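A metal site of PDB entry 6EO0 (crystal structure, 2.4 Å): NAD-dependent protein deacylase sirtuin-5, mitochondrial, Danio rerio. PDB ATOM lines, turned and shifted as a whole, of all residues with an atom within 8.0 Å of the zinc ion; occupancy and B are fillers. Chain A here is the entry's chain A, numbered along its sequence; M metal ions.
The backbone NH (N) of Glu 146 lies close to the side-chain sulfur (SG) of Cys 144, 3.8 Å away.
N of Cys 182 lies within hydrogen-bond range of O of Gly 189 (2.9 Å).
N of Arg 184 lies close to SG of Cys 182, 3.6 Å away.
The backbone carbonyl oxygen (O) of Cys 182 is in hydrogen-bond range of the side-chain amide nitrogen (ND2) of Asn 188, at 3.2 Å.
SG of Cys 141 lies close to N of Ser 143 (3.3 Å).
The backbone NH (N) of Cys 141 is in hydrogen-bond range of the backbone carbonyl oxygen (O) of Glu 146, 3.1 Å away.
The side-chain sulfur of Cys 187 lies close to the backbone NH of Gly 189 (3.5 Å).
Within 4 Å of the zinc ion: Cys 141, Cys 144, Cys 182 and Cys 187.
Along chain A the residues within 4 Å of the zinc ion span positions 141 to 187.
The nearest printed residue that does not touch the zinc ion is Gly 189 (4.5 Å).
The zinc ion is bound by the side-chain sulfur of Cys 144, the side-chain sulfur of Cys 182, the side-chain sulfur of Cys 141 and the side-chain sulfur of Cys 187.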
ATOM      1  N   ARG A 140      28.389 -19.047  -1.497  1.00  0.00           N
ATOM      2  CA  ARG A 140      28.007 -18.778  -2.886  1.00  0.00           C
ATOM      3  C   ARG A 140      27.042 -17.641  -2.880  1.00  0.00           C
ATOM      4  O   ARG A 140      26.158 -17.602  -2.030  1.00  0.00           O
ATOM      5  CB  ARG A 140      27.322 -19.972  -3.526  1.00  0.00           C
ATOM      6  CG  ARG A 140      27.054 -19.835  -5.045  1.00  0.00           C
ATOM      7  CD  ARG A 140      25.941 -20.697  -5.579  1.00  0.00           C
ATOM      8  NE  ARG A 140      25.997 -22.032  -4.973  1.00  0.00           N
ATOM      9  CZ  ARG A 140      25.058 -22.968  -5.038  1.00  0.00           C
ATOM     10  NH1 ARG A 140      25.212 -24.116  -4.360  1.00  0.00           N
ATOM     11  NH2 ARG A 140      23.936 -22.764  -5.740  1.00  0.00           N
ATOM     12  N   CYS A 141      27.176 -16.715  -3.826  1.00  0.00           N
ATOM     13  CA  CYS A 141      26.315 -15.540  -3.885  1.00  0.00           C
ATOM     14  C   CYS A 141      25.057 -15.850  -4.671  1.00  0.00           C
ATOM     15  O   CYS A 141      25.107 -16.419  -5.761  1.00  0.00           O
ATOM     16  CB  CYS A 141      27.037 -14.329  -4.466  1.00  0.00           C
ATOM     17  SG  CYS A 141      26.005 -12.829  -4.770  1.00  0.00           S
ATOM     18  N   MET A 142      23.924 -15.452  -4.101  1.00  0.00           N
ATOM     19  CA  MET A 142      22.603 -15.618  -4.695  1.00  0.00           C
ATOM     20  C   MET A 142      22.367 -14.733  -5.910  1.00  0.00           C
ATOM     21  O   MET A 142      21.502 -15.043  -6.720  1.00  0.00           O
ATOM     22  CB  MET A 142      21.517 -15.293  -3.647  1.00  0.00           C
ATOM     23  CG  MET A 142      21.448 -16.228  -2.460  1.00  0.00           C
ATOM     24  SD  MET A 142      20.607 -17.790  -2.796  1.00  0.00           S
ATOM     25  CE  MET A 142      19.015 -17.524  -3.593  1.00  0.00           C
ATOM     26  N   SER A 143      23.077 -13.615  -6.032  1.00  0.00           N
ATOM     27  CA  SER A 143      22.935 -12.758  -7.202  1.00  0.00           C
ATOM     28  C   SER A 143      23.980 -13.160  -8.245  1.00  0.00           C
ATOM     29  O   SER A 143      23.625 -13.650  -9.318  1.00  0.00           O
ATOM     30  CB  SER A 143      23.104 -11.279  -6.838  1.00  0.00           C
ATOM     31  OG  SER A 143      22.323 -10.944  -5.709  1.00  0.00           O
ATOM     32  N   CYS A 144      25.257 -12.980  -7.903  1.00  0.00           N
ATOM     33  CA  CYS A 144      26.330 -13.035  -8.898  1.00  0.00           C
ATOM     34  C   CYS A 144      27.018 -14.409  -9.028  1.00  0.00           C
ATOM     35  O   CYS A 144      27.666 -14.675 -10.025  1.00  0.00           O
ATOM     36  CB  CYS A 144      27.345 -11.939  -8.604  1.00  0.00           C
ATOM     37  SG  CYS A 144      28.466 -12.245  -7.234  1.00  0.00           S
ATOM     38  N   GLY A 145      26.871 -15.283  -8.040  1.00  0.00           N
ATOM     39  CA  GLY A 145      27.419 -16.630  -8.109  1.00  0.00           C
ATOM     40  C   GLY A 145      28.854 -16.854  -7.687  1.00  0.00           C
ATOM     41  O   GLY A 145      29.403 -17.938  -7.884  1.00  0.00           O
ATOM     42  N   GLU A 146      29.486 -15.867  -7.081  1.00  0.00           N
ATOM     43  CA  GLU A 146      30.867 -16.033  -6.636  1.00  0.00           C
ATOM     44  C   GLU A 146      30.933 -17.085  -5.545  1.00  0.00           C
ATOM     45  O   GLU A 146      30.200 -17.003  -4.571  1.00  0.00           O
ATOM     46  CB  GLU A 146      31.457 -14.737  -6.125  1.00  0.00           C
ATOM     47  CG  GLU A 146      32.974 -14.822  -5.974  1.00  0.00           C
ATOM     48  CD  GLU A 146      33.598 -13.577  -5.346  1.00  0.00           C
ATOM     49  OE1 GLU A 146      34.839 -13.509  -5.191  1.00  0.00           O
ATOM     50  OE2 GLU A 146      32.852 -12.655  -4.994  1.00  0.00           O
ATOM     51  N   LYS A 148      33.550 -18.326  -2.819  1.00  0.00           N
ATOM     52  CA  LYS A 148      34.775 -18.001  -2.067  1.00  0.00           C
ATOM     53  C   LYS A 148      34.861 -18.988  -0.948  1.00  0.00           C
ATOM     54  O   LYS A 148      33.832 -19.497  -0.489  1.00  0.00           O
ATOM     55  CB  LYS A 148      34.696 -16.596  -1.426  1.00  0.00           C
ATOM     56  CG  LYS A 148      34.477 -15.435  -2.395  1.00  0.00           C
ATOM     57  CD  LYS A 148      34.362 -14.088  -1.681  1.00  0.00           C
ATOM     58  CE  LYS A 148      32.969 -13.894  -1.072  1.00  0.00           C
ATOM     59  NZ  LYS A 148      32.047 -12.872  -1.700  1.00  0.00           N
ATOM     60  N   ARG A 181      26.845 -11.205   3.483  1.00  0.00           N
ATOM     61  CA  ARG A 181      26.631 -10.535   2.176  1.00  0.00           C
ATOM     62  C   ARG A 181      27.863 -10.648   1.295  1.00  0.00           C
ATOM     63  O   ARG A 181      28.999 -10.676   1.778  1.00  0.00           O
ATOM     64  CB  ARG A 181      26.265  -9.043   2.349  1.00  0.00           C
ATOM     65  CG  ARG A 181      25.092  -8.707   3.265  1.00  0.00           C
ATOM     66  CD  ARG A 181      23.853  -9.572   2.990  1.00  0.00           C
ATOM     67  NE  ARG A 181      22.436  -9.342   2.660  1.00  0.00           N
ATOM     68  CZ  ARG A 181      21.894  -9.103   1.468  1.00  0.00           C
ATOM     69  NH1 ARG A 181      22.644  -8.741   0.442  1.00  0.00           N
ATOM     70  NH2 ARG A 181      20.578  -9.021   1.384  1.00  0.00           N
ATOM     71  N   CYS A 182      27.616 -10.725  -0.012  1.00  0.00           N
ATOM     72  CA  CYS A 182      28.679 -10.757  -1.022  1.00  0.00           C
ATOM     73  C   CYS A 182      29.568  -9.512  -0.910  1.00  0.00           C
ATOM     74  O   CYS A 182      29.082  -8.373  -0.985  1.00  0.00           O
ATOM     75  CB  CYS A 182      28.064 -10.851  -2.396  1.00  0.00           C
ATOM     76  SG  CYS A 182      29.077 -10.805  -3.832  1.00  0.00           S
ATOM     77  N   GLU A 183      30.852  -9.749  -0.710  1.00  0.00           N
ATOM     78  CA  GLU A 183      31.857  -8.720  -0.572  1.00  0.00           C
ATOM     79  C   GLU A 183      32.086  -7.898  -1.853  1.00  0.00           C
ATOM     80  O   GLU A 183      32.830  -6.909  -1.805  1.00  0.00           O
ATOM     81  CB  GLU A 183      33.220  -9.371  -0.222  1.00  0.00           C
ATOM     82  CG  GLU A 183      33.359 -10.250   1.011  1.00  0.00           C
ATOM     83  CD  GLU A 183      33.794  -9.465   2.245  1.00  0.00           C
ATOM     84  OE1 GLU A 183      35.013  -9.277   2.520  1.00  0.00           O
ATOM     85  OE2 GLU A 183      32.841  -8.971   2.911  1.00  0.00           O
ATOM     86  N   ARG A 184      31.484  -8.280  -2.989  1.00  0.00           N
ATOM     87  CA  ARG A 184      31.506  -7.468  -4.192  1.00  0.00           C
ATOM     88  C   ARG A 184      30.577  -6.287  -4.018  1.00  0.00           C
ATOM     89  O   ARG A 184      29.356  -6.398  -4.112  1.00  0.00           O
ATOM     90  CB  ARG A 184      31.044  -8.253  -5.441  1.00  0.00           C
ATOM     91  CG  ARG A 184      32.107  -8.920  -6.346  1.00  0.00           C
ATOM     92  CD  ARG A 184      31.644  -8.951  -7.807  1.00  0.00           C
ATOM     93  NE  ARG A 184      32.488  -9.878  -8.530  1.00  0.00           N
ATOM     94  CZ  ARG A 184      33.712  -9.633  -9.005  1.00  0.00           C
ATOM     95  NH1 ARG A 184      34.296  -8.442  -8.871  1.00  0.00           N
ATOM     96  NH2 ARG A 184      34.381 -10.601  -9.640  1.00  0.00           N
ATOM     97  N   LYS A 185      31.162  -5.120  -3.807  1.00  0.00           N
ATOM     98  CA  LYS A 185      30.412  -3.854  -3.849  1.00  0.00           C
ATOM     99  C   LYS A 185      29.795  -3.639  -5.269  1.00  0.00           C
ATOM    100  O   LYS A 185      30.415  -4.054  -6.276  1.00  0.00           O
ATOM    101  CB  LYS A 185      31.340  -2.700  -3.407  1.00  0.00           C
ATOM    102  CG  LYS A 185      31.041  -2.250  -2.016  1.00  0.00           C
ATOM    103  CD  LYS A 185      32.173  -1.377  -1.478  1.00  0.00           C
ATOM    104  CE  LYS A 185      31.848  -0.872  -0.080  1.00  0.00           C
ATOM    105  NZ  LYS A 185      32.252   0.550   0.084  1.00  0.00           N
ATOM    106  N   SER A 186      28.564  -3.175  -5.342  1.00  0.00           N
ATOM    107  CA  SER A 186      27.818  -3.205  -6.600  1.00  0.00           C
ATOM    108  C   SER A 186      27.160  -4.549  -6.903  1.00  0.00           C
ATOM    109  O   SER A 186      26.362  -4.638  -7.886  1.00  0.00           O
ATOM    110  CB  SER A 186      28.621  -2.784  -7.821  1.00  0.00           C
ATOM    111  OG  SER A 186      29.314  -1.589  -7.558  1.00  0.00           O
ATOM    112  N   CYS A 187      27.321  -5.550  -6.056  1.00  0.00           N
ATOM    113  CA  CYS A 187      26.356  -6.662  -6.003  1.00  0.00           C
ATOM    114  C   CYS A 187      25.603  -6.660  -4.698  1.00  0.00           C
ATOM    115  O   CYS A 187      24.397  -6.794  -4.733  1.00  0.00           O
ATOM    116  CB  CYS A 187      27.099  -7.995  -6.155  1.00  0.00           C
ATOM    117  SG  CYS A 187      26.043  -9.425  -6.020  1.00  0.00           S
ATOM    118  N   ASN A 188      26.341  -6.581  -3.570  1.00  0.00           N
ATOM    119  CA  ASN A 188      25.857  -6.858  -2.199  1.00  0.00           C
ATOM    120  C   ASN A 188      24.663  -7.868  -2.044  1.00  0.00           C
ATOM    121  O   ASN A 188      23.688  -7.630  -1.310  1.00  0.00           O
ATOM    122  CB  ASN A 188      25.583  -5.533  -1.427  1.00  0.00           C
ATOM    123  CG  ASN A 188      25.981  -5.603   0.063  1.00  0.00           C
ATOM    124  OD1 ASN A 188      25.251  -5.141   0.935  1.00  0.00           O
ATOM    125  ND2 ASN A 188      27.139  -6.181   0.350  1.00  0.00           N
ATOM    126  N   GLY A 189      24.762  -8.990  -2.762  1.00  0.00           N
ATOM    127  CA  GLY A 189      23.764 -10.047  -2.678  1.00  0.00           C
ATOM    128  C   GLY A 189      23.807 -10.848  -1.380  1.00  0.00           C
ATOM    129  O   GLY A 189      24.802 -10.780  -0.633  1.00  0.00           O
ATOM    130  N   LEU A 190      22.727 -11.586  -1.114  1.00  0.00           N
ATOM    131  CA  LEU A 190      22.666 -12.545   0.008  1.00  0.00           C
ATOM    132  C   LEU A 190      23.536 -13.806  -0.303  1.00  0.00           C
ATOM    133  O   LEU A 190      23.368 -14.461  -1.331  1.00  0.00           O
ATOM    134  CB  LEU A 190      21.216 -12.972   0.252  1.00  0.00           C
ATOM    135  CG  LEU A 190      20.997 -14.013   1.393  1.00  0.00           C
ATOM    136  CD1 LEU A 190      21.642 -13.585   2.702  1.00  0.00           C
ATOM    137  CD2 LEU A 190      19.522 -14.344   1.555  1.00  0.00           C
ATOM    138  N   LEU A 191      24.467 -14.120   0.590  1.00  0.00           N
ATOM    139  CA  LEU A 191      25.223 -15.366   0.464  1.00  0.00           C
ATOM    140  C   LEU A 191      24.423 -16.566   0.970  1.00  0.00           C
ATOM    141  O   LEU A 191      23.625 -16.443   1.922  1.00  0.00           O
ATOM    142  CB  LEU A 191      26.547 -15.244   1.241  1.00  0.00           C
ATOM    143  CG  LEU A 191      27.503 -14.156   0.744  1.00  0.00           C
ATOM    144  CD1 LEU A 191      28.823 -14.124   1.486  1.00  0.00           C
ATOM    145  CD2 LEU A 191      27.744 -14.299  -0.723  1.00  0.00           C
HETATM  146 ZN    ZN M   1      27.515 -11.196  -5.485  1.00  0.00          ZN
